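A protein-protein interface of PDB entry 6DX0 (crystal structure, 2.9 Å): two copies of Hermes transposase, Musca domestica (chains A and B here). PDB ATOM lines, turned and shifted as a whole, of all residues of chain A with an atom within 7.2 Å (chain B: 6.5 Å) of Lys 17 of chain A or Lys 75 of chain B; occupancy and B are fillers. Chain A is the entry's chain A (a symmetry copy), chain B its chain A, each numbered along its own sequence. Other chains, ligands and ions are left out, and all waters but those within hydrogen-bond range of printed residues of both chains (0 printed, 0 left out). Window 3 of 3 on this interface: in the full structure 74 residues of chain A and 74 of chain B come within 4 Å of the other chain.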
ATOM      1  N   VAL A  11     -19.201 -23.401   5.354  1.00  0.00           N
ATOM      2  CA  VAL A  11     -17.893 -23.725   4.803  1.00  0.00           C
ATOM      3  C   VAL A  11     -17.103 -22.447   4.588  1.00  0.00           C
ATOM      4  O   VAL A  11     -17.651 -21.346   4.498  1.00  0.00           O
ATOM      5  CB  VAL A  11     -17.992 -24.522   3.484  1.00  0.00           C
ATOM      6  CG1 VAL A  11     -18.829 -25.771   3.673  1.00  0.00           C
ATOM      7  CG2 VAL A  11     -18.546 -23.651   2.370  1.00  0.00           C
ATOM      8  N   SER A  12     -15.791 -22.614   4.466  1.00  0.00           N
ATOM      9  CA  SER A  12     -14.905 -21.477   4.287  1.00  0.00           C
ATOM     10  C   SER A  12     -15.211 -20.758   2.982  1.00  0.00           C
ATOM     11  O   SER A  12     -15.789 -21.320   2.049  1.00  0.00           O
ATOM     12  CB  SER A  12     -13.444 -21.924   4.301  1.00  0.00           C
ATOM     13  OG  SER A  12     -13.204 -22.908   3.313  1.00  0.00           O
ATOM     14  N   ALA A  13     -14.809 -19.487   2.932  1.00  0.00           N
ATOM     15  CA  ALA A  13     -15.035 -18.673   1.743  1.00  0.00           C
ATOM     16  C   ALA A  13     -14.311 -19.250   0.536  1.00  0.00           C
ATOM     17  O   ALA A  13     -14.894 -19.392  -0.544  1.00  0.00           O
ATOM     18  CB  ALA A  13     -14.590 -17.237   2.003  1.00  0.00           C
ATOM     19  N   ASP A  14     -13.033 -19.589   0.700  1.00  0.00           N
ATOM     20  CA  ASP A  14     -12.267 -20.162  -0.398  1.00  0.00           C
ATOM     21  C   ASP A  14     -12.761 -21.553  -0.794  1.00  0.00           C
ATOM     22  O   ASP A  14     -12.442 -22.019  -1.894  1.00  0.00           O
ATOM     23  CB  ASP A  14     -10.782 -20.197  -0.017  1.00  0.00           C
ATOM     24  CG  ASP A  14     -10.216 -18.807   0.248  1.00  0.00           C
ATOM     25  OD1 ASP A  14      -8.977 -18.652   0.248  1.00  0.00           O
ATOM     26  OD2 ASP A  14     -11.015 -17.866   0.451  1.00  0.00           O
ATOM     27  N   CYS A  15     -13.536 -22.223   0.067  1.00  0.00           N
ATOM     28  CA  CYS A  15     -14.139 -23.499  -0.306  1.00  0.00           C
ATOM     29  C   CYS A  15     -15.332 -23.300  -1.235  1.00  0.00           C
ATOM     30  O   CYS A  15     -15.465 -23.997  -2.248  1.00  0.00           O
ATOM     31  CB  CYS A  15     -14.569 -24.265   0.944  1.00  0.00           C
ATOM     32  SG  CYS A  15     -15.900 -25.457   0.675  1.00  0.00           S
ATOM     33  N   LYS A  16     -16.211 -22.351  -0.903  1.00  0.00           N
ATOM     34  CA  LYS A  16     -17.410 -22.129  -1.705  1.00  0.00           C
ATOM     35  C   LYS A  16     -17.083 -21.523  -3.067  1.00  0.00           C
ATOM     36  O   LYS A  16     -17.826 -21.738  -4.030  1.00  0.00           O
ATOM     37  CB  LYS A  16     -18.378 -21.242  -0.930  1.00  0.00           C
ATOM     38  CG  LYS A  16     -19.769 -21.155  -1.511  1.00  0.00           C
ATOM     39  CD  LYS A  16     -20.561 -20.105  -0.760  1.00  0.00           C
ATOM     40  CE  LYS A  16     -19.744 -18.824  -0.624  1.00  0.00           C
ATOM     41  NZ  LYS A  16     -20.324 -17.876   0.368  1.00  0.00           N
ATOM     42  N   LYS A  17     -15.982 -20.771  -3.176  1.00  0.00           N
ATOM     43  CA  LYS A  17     -15.518 -20.335  -4.490  1.00  0.00           C
ATOM     44  C   LYS A  17     -15.229 -21.520  -5.406  1.00  0.00           C
ATOM     45  O   LYS A  17     -15.249 -21.366  -6.631  1.00  0.00           O
ATOM     46  CB  LYS A  17     -14.277 -19.441  -4.349  1.00  0.00           C
ATOM     47  CG  LYS A  17     -13.643 -18.998  -5.674  1.00  0.00           C
ATOM     48  CD  LYS A  17     -14.658 -18.287  -6.579  1.00  0.00           C
ATOM     49  CE  LYS A  17     -14.188 -18.206  -8.033  1.00  0.00           C
ATOM     50  NZ  LYS A  17     -13.005 -17.310  -8.232  1.00  0.00           N
ATOM     51  N   GLU A  18     -14.984 -22.703  -4.840  1.00  0.00           N
ATOM     52  CA  GLU A  18     -14.818 -23.912  -5.632  1.00  0.00           C
ATOM     53  C   GLU A  18     -16.115 -24.699  -5.806  1.00  0.00           C
ATOM     54  O   GLU A  18     -16.171 -25.589  -6.659  1.00  0.00           O
ATOM     55  CB  GLU A  18     -13.738 -24.815  -5.018  1.00  0.00           C
ATOM     56  CG  GLU A  18     -13.284 -25.927  -5.958  1.00  0.00           C
ATOM     57  CD  GLU A  18     -11.833 -26.312  -5.792  1.00  0.00           C
ATOM     58  OE1 GLU A  18     -11.431 -26.657  -4.660  1.00  0.00           O
ATOM     59  OE2 GLU A  18     -11.099 -26.270  -6.806  1.00  0.00           O
ATOM     60  N   ALA A  19     -17.159 -24.402  -5.028  1.00  0.00           N
ATOM     61  CA  ALA A  19     -18.478 -24.947  -5.341  1.00  0.00           C
ATOM     62  C   ALA A  19     -19.031 -24.310  -6.619  1.00  0.00           C
ATOM     63  O   ALA A  19     -19.297 -25.000  -7.611  1.00  0.00           O
ATOM     64  CB  ALA A  19     -19.427 -24.742  -4.158  1.00  0.00           C
ATOM     65  N   ILE A  20     -19.169 -22.983  -6.634  1.00  0.00           N
ATOM     66  CA  ILE A  20     -19.528 -22.278  -7.859  1.00  0.00           C
ATOM     67  C   ILE A  20     -18.484 -22.442  -8.956  1.00  0.00           C
ATOM     68  O   ILE A  20     -18.734 -22.052 -10.096  1.00  0.00           O
ATOM     69  CB  ILE A  20     -19.763 -20.772  -7.595  1.00  0.00           C
ATOM     70  CG1 ILE A  20     -18.448 -19.990  -7.712  1.00  0.00           C
ATOM     71  CG2 ILE A  20     -20.394 -20.561  -6.235  1.00  0.00           C
ATOM     72  CD1 ILE A  20     -18.507 -18.578  -7.150  1.00  0.00           C
ATOM     73  N   GLU A  21     -17.309 -22.979  -8.641  1.00  0.00           N
ATOM     74  CA  GLU A  21     -16.339 -23.294  -9.680  1.00  0.00           C
ATOM     75  C   GLU A  21     -16.593 -24.665 -10.275  1.00  0.00           C
ATOM     76  O   GLU A  21     -16.337 -24.872 -11.466  1.00  0.00           O
ATOM     77  CB  GLU A  21     -14.911 -23.219  -9.124  1.00  0.00           C
ATOM     78  CG  GLU A  21     -13.782 -23.326 -10.152  1.00  0.00           C
ATOM     79  CD  GLU A  21     -12.402 -23.451  -9.500  1.00  0.00           C
ATOM     80  OE1 GLU A  21     -11.675 -24.420  -9.818  1.00  0.00           O
ATOM     81  OE2 GLU A  21     -12.049 -22.592  -8.659  1.00  0.00           O
ATOM     82  N   LYS A  22     -17.112 -25.596  -9.476  1.00  0.00           N
ATOM     83  CA  LYS A  22     -17.396 -26.948  -9.941  1.00  0.00           C
ATOM     84  C   LYS A  22     -18.830 -27.106 -10.430  1.00  0.00           C
ATOM     85  O   LYS A  22     -19.110 -28.000 -11.240  1.00  0.00           O
ATOM     86  CB  LYS A  22     -17.118 -27.970  -8.823  1.00  0.00           C
ATOM     87  CG  LYS A  22     -15.647 -28.073  -8.405  1.00  0.00           C
ATOM     88  CD  LYS A  22     -14.919 -29.262  -9.035  1.00  0.00           C
ATOM     89  CE  LYS A  22     -13.725 -28.818  -9.877  1.00  0.00           C
ATOM     90  NZ  LYS A  22     -12.918 -27.756  -9.221  1.00  0.00           N
ATOM     91  N   ALA A  24     -20.579 -24.520 -12.053  1.00  0.00           N
ATOM     92  CA  ALA A  24     -20.544 -23.929 -13.383  1.00  0.00           C
ATOM     93  C   ALA A  24     -19.788 -24.788 -14.384  1.00  0.00           C
ATOM     94  O   ALA A  24     -19.840 -24.500 -15.581  1.00  0.00           O
ATOM     95  CB  ALA A  24     -19.928 -22.531 -13.329  1.00  0.00           C
ATOM     96  N   PHE B  48     -16.061 -33.287  -5.787  1.00  0.00           N
ATOM     97  CA  PHE B  48     -15.901 -32.140  -4.911  1.00  0.00           C
ATOM     98  C   PHE B  48     -16.775 -32.243  -3.669  1.00  0.00           C
ATOM     99  O   PHE B  48     -16.389 -31.754  -2.605  1.00  0.00           O
ATOM    100  CB  PHE B  48     -16.217 -30.867  -5.670  1.00  0.00           C
ATOM    101  CG  PHE B  48     -16.220 -29.653  -4.808  1.00  0.00           C
ATOM    102  CD1 PHE B  48     -15.036 -29.031  -4.469  1.00  0.00           C
ATOM    103  CD2 PHE B  48     -17.407 -29.135  -4.326  1.00  0.00           C
ATOM    104  CE1 PHE B  48     -15.037 -27.917  -3.672  1.00  0.00           C
ATOM    105  CE2 PHE B  48     -17.414 -28.021  -3.527  1.00  0.00           C
ATOM    106  CZ  PHE B  48     -16.228 -27.412  -3.200  1.00  0.00           C
ATOM    107  N   ILE B  70     -28.701 -17.759 -10.428  1.00  0.00           N
ATOM    108  CA  ILE B  70     -28.325 -16.421 -10.874  1.00  0.00           C
ATOM    109  C   ILE B  70     -26.814 -16.249 -10.842  1.00  0.00           C
ATOM    110  O   ILE B  70     -26.220 -15.715 -11.786  1.00  0.00           O
ATOM    111  CB  ILE B  70     -29.038 -15.369 -10.011  1.00  0.00           C
ATOM    112  CG1 ILE B  70     -28.437 -13.981 -10.226  1.00  0.00           C
ATOM    113  CG2 ILE B  70     -28.931 -15.772  -8.563  1.00  0.00           C
ATOM    114  CD1 ILE B  70     -28.513 -13.463 -11.641  1.00  0.00           C
ATOM    115  N   THR B  71     -26.160 -16.699  -9.764  1.00  0.00           N
ATOM    116  CA  THR B  71     -24.707 -16.564  -9.721  1.00  0.00           C
ATOM    117  C   THR B  71     -24.045 -17.550 -10.677  1.00  0.00           C
ATOM    118  O   THR B  71     -23.135 -17.174 -11.424  1.00  0.00           O
ATOM    119  CB  THR B  71     -24.160 -16.723  -8.290  1.00  0.00           C
ATOM    120  OG1 THR B  71     -24.801 -17.807  -7.603  1.00  0.00           O
ATOM    121  CG2 THR B  71     -24.334 -15.426  -7.499  1.00  0.00           C
ATOM    122  N   LEU B  72     -24.494 -18.812 -10.679  1.00  0.00           N
ATOM    123  CA  LEU B  72     -24.060 -19.755 -11.712  1.00  0.00           C
ATOM    124  C   LEU B  72     -24.133 -19.112 -13.091  1.00  0.00           C
ATOM    125  O   LEU B  72     -23.206 -19.233 -13.904  1.00  0.00           O
ATOM    126  CB  LEU B  72     -24.910 -21.029 -11.675  1.00  0.00           C
ATOM    127  CG  LEU B  72     -24.613 -22.014 -10.541  1.00  0.00           C
ATOM    128  CD1 LEU B  72     -25.049 -23.445 -10.902  1.00  0.00           C
ATOM    129  CD2 LEU B  72     -23.133 -21.968 -10.161  1.00  0.00           C
ATOM    130  N   SER B  73     -25.232 -18.405 -13.365  1.00  0.00           N
ATOM    131  CA  SER B  73     -25.284 -17.598 -14.576  1.00  0.00           C
ATOM    132  C   SER B  73     -24.143 -16.593 -14.612  1.00  0.00           C
ATOM    133  O   SER B  73     -23.534 -16.369 -15.665  1.00  0.00           O
ATOM    134  CB  SER B  73     -26.619 -16.867 -14.682  1.00  0.00           C
ATOM    135  OG  SER B  73     -26.502 -15.806 -15.617  1.00  0.00           O
ATOM    136  N   ARG B  74     -23.841 -15.970 -13.474  1.00  0.00           N
ATOM    137  CA  ARG B  74     -22.860 -14.901 -13.516  1.00  0.00           C
ATOM    138  C   ARG B  74     -21.442 -15.439 -13.520  1.00  0.00           C
ATOM    139  O   ARG B  74     -20.538 -14.748 -13.995  1.00  0.00           O
ATOM    140  CB  ARG B  74     -23.094 -13.923 -12.359  1.00  0.00           C
ATOM    141  CG  ARG B  74     -24.365 -13.107 -12.553  1.00  0.00           C
ATOM    142  CD  ARG B  74     -24.483 -11.857 -11.693  1.00  0.00           C
ATOM    143  NE  ARG B  74     -25.179 -12.115 -10.435  1.00  0.00           N
ATOM    144  CZ  ARG B  74     -26.007 -11.261  -9.826  1.00  0.00           C
ATOM    145  NH1 ARG B  74     -26.282 -10.074 -10.360  1.00  0.00           N
ATOM    146  NH2 ARG B  74     -26.569 -11.599  -8.665  1.00  0.00           N
ATOM    147  N   LYS B  75     -21.236 -16.672 -13.049  1.00  0.00           N
ATOM    148  CA  LYS B  75     -19.897 -17.251 -13.059  1.00  0.00           C
ATOM    149  C   LYS B  75     -19.493 -17.710 -14.454  1.00  0.00           C
ATOM    150  O   LYS B  75     -18.345 -17.495 -14.866  1.00  0.00           O
ATOM    151  CB  LYS B  75     -19.808 -18.420 -12.078  1.00  0.00           C
ATOM    152  CG  LYS B  75     -18.379 -18.938 -11.851  1.00  0.00           C
ATOM    153  CD  LYS B  75     -17.587 -18.050 -10.884  1.00  0.00           C
ATOM    154  CE  LYS B  75     -16.196 -17.707 -11.417  1.00  0.00           C
ATOM    155  NZ  LYS B  75     -15.291 -18.888 -11.520  1.00  0.00           N
ATOM    156  N   VAL B  76     -20.416 -18.355 -15.186  1.00  0.00           N
ATOM    157  CA  VAL B  76     -20.117 -18.749 -16.563  1.00  0.00           C
ATOM    158  C   VAL B  76     -19.825 -17.517 -17.393  1.00  0.00           C
ATOM    159  O   VAL B  76     -18.946 -17.528 -18.264  1.00  0.00           O
ATOM    160  CB  VAL B  76     -21.264 -19.576 -17.179  1.00  0.00           C
ATOM    161  CG1 VAL B  76     -21.499 -20.827 -16.393  1.00  0.00           C
ATOM    162  CG2 VAL B  76     -22.536 -18.771 -17.253  1.00  0.00           C
ATOM    163  N   THR B  77     -20.549 -16.430 -17.117  1.00  0.00           N
ATOM    164  CA  THR B  77     -20.265 -15.162 -17.769  1.00  0.00           C
ATOM    165  C   THR B  77     -18.890 -14.648 -17.364  1.00  0.00           C
ATOM    166  O   THR B  77     -18.135 -14.142 -18.202  1.00  0.00           O
ATOM    167  CB  THR B  77     -21.358 -14.154 -17.419  1.00  0.00           C
ATOM    168  OG1 THR B  77     -22.637 -14.687 -17.793  1.00  0.00           O
ATOM    169  CG2 THR B  77     -21.140 -12.868 -18.164  1.00  0.00           C
ATOM    170  N   SER B  78     -18.538 -14.799 -16.083  1.00  0.00           N
ATOM    171  CA  SER B  78     -17.215 -14.395 -15.616  1.00  0.00           C
ATOM    172  C   SER B  78     -16.138 -15.319 -16.162  1.00  0.00           C
ATOM    173  O   SER B  78     -15.160 -14.861 -16.765  1.00  0.00           O
ATOM    174  CB  SER B  78     -17.181 -14.378 -14.091  1.00  0.00           C
ATOM    175  OG  SER B  78     -18.074 -13.409 -13.576  1.00  0.00           O
ATOM    176  N   ASP B  79     -16.299 -16.626 -15.961  1.00  0.00           N
ATOM    177  CA  ASP B  79     -15.283 -17.568 -16.408  1.00  0.00           C
ATOM    178  C   ASP B  79     -15.129 -17.559 -17.921  1.00  0.00           C
ATOM    179  O   ASP B  79     -14.073 -17.946 -18.437  1.00  0.00           O
ATOM    180  CB  ASP B  79     -15.626 -18.971 -15.912  1.00  0.00           C
ATOM    181  CG  ASP B  79     -14.404 -19.862 -15.792  1.00  0.00           C
ATOM    182  OD1 ASP B  79     -13.639 -19.702 -14.814  1.00  0.00           O
ATOM    183  OD2 ASP B  79     -14.210 -20.726 -16.667  1.00  0.00           O
ATOM    184  N   ALA B  80     -16.162 -17.123 -18.639  1.00  0.00           N
ATOM    185  CA  ALA B  80     -16.066 -17.001 -20.086  1.00  0.00           C
ATOM    186  C   ALA B  80     -14.877 -16.133 -20.470  1.00  0.00           C
ATOM    187  O   ALA B  80     -13.946 -16.592 -21.137  1.00  0.00           O
ATOM    188  CB  ALA B  80     -17.364 -16.422 -20.648  1.00  0.00           C
ATOM    189  N   GLU B  82     -12.383 -15.077 -18.751  1.00  0.00           N
ATOM    190  CA  GLU B  82     -11.147 -15.664 -18.252  1.00  0.00           C
ATOM    191  C   GLU B  82     -10.554 -16.642 -19.261  1.00  0.00           C
ATOM    192  O   GLU B  82      -9.452 -16.430 -19.779  1.00  0.00           O
ATOM    193  CB  GLU B  82     -11.426 -16.358 -16.919  1.00  0.00           C
ATOM    194  CG  GLU B  82     -10.199 -16.661 -16.089  1.00  0.00           C
ATOM    195  CD  GLU B  82     -10.505 -17.599 -14.936  1.00  0.00           C
ATOM    196  OE1 GLU B  82     -10.366 -18.829 -15.115  1.00  0.00           O
ATOM    197  OE2 GLU B  82     -10.898 -17.109 -13.855  1.00  0.00           O
ATOM    198  N   LEU B 505     -17.132 -22.303 -23.568  1.00  0.00           N
ATOM    199  CA  LEU B 505     -16.710 -23.061 -22.403  1.00  0.00           C
ATOM    200  C   LEU B 505     -16.734 -24.550 -22.726  1.00  0.00           C
ATOM    201  O   LEU B 505     -15.665 -25.144 -22.885  1.00  0.00           O
ATOM    202  CB  LEU B 505     -17.570 -22.696 -21.182  1.00  0.00           C
ATOM    203  CG  LEU B 505     -16.891 -21.685 -20.213  1.00  0.00           C
ATOM    204  CD1 LEU B 505     -15.778 -20.852 -20.871  1.00  0.00           C
ATOM    205  CD2 LEU B 505     -17.886 -20.749 -19.516  1.00  0.00           C
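Lys 17 of chain A touches one residue of chain B.
Printed residues of chain B within 4 Å of Ala 19 of chain A: Phe 48 (3.6 Å).
Of the printed residues of chain A, Phe 48 of chain B touches Cys 15, Glu 18, Ala 19 and Lys 22.
Printed residues of chain B within 4 Å of Lys 22 of chain A: Phe 48 (3.9 Å).
Of the printed residues of chain B, Glu 18 of chain A touches Phe 48 (3.5 Å).
The nearest residue of chain B that does not touch Lys 17 of chain A is Glu 82 of chain B (6.0 Å).
The nearest residue of chain A that does not touch Lys 75 of chain B is Ala 24 of chain A (4.2 Å).
The nearest printed residue of chain A that does not touch Phe 48 of chain B is Lys 16 of chain A (5.6 Å).
No position is printed for both chains.
Of the 7 pairs that touch across the chains among the printed residues, none has its exchanged pair printed and touching as well.
The side-chain hydroxyl (OG) of Ser 12 of chain A lies close to the backbone NH (N) of Cys 15 of chain A.
NZ of Lys 22 of chain A is in salt-bridge range of OE1 of Glu 21 of chain A, 3.6 Å away.
The side-chain carboxylate (OE2) of Glu 18 of chain A lies within salt-bridge range of the side-chain amino group (NZ) of Lys 22 of chain A.
OD1 of Asp 79 of chain B lies within salt-bridge range of NZ of Lys 75 of chain B (3.8 Å).
Phe 48 of chain B touches Cys 15 of chain A.
Lys 17 of chain A touches Lys 75 of chain B (CE to NZ, 3.7 Å).
Glu 18 of chain A touches Phe 48 of chain B.
Phe 48 of chain B touches Ala 19 of chain A.
Lys 75 of chain B touches Ile 20 of chain A (CG to O, 3.6 Å).
Phe 48 of chain B touches Lys 22 of chain A (CB to CD, 3.9 Å).
Val 76 of chain B touches Ala 24 of chain A (CG1 to CB, 3.8 Å).
Of the 14 printed residues of chain B, 3 touch a printed residue of chain A.
Printed residues of chain B that touch a printed residue of chain A: Phe 48, Lys 75 and Val 76.
Of the 13 printed residues of chain A, 7 touch a printed residue of chain B.
Printed residues of chain A that touch a printed residue of chain B: Cys 15, Lys 17, Glu 18, Ala 19, Ile 20, Lys 22 and Ala 24.
Hydrophobic or aromatic side chains of chain A that line the printed part of chain B: Ala 19, Ile 20 and Ala 24.
Among the printed residues, no Asp or Glu carboxylate lies within 4 Å of a Lys or Arg side-chain nitrogen of the other chain.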
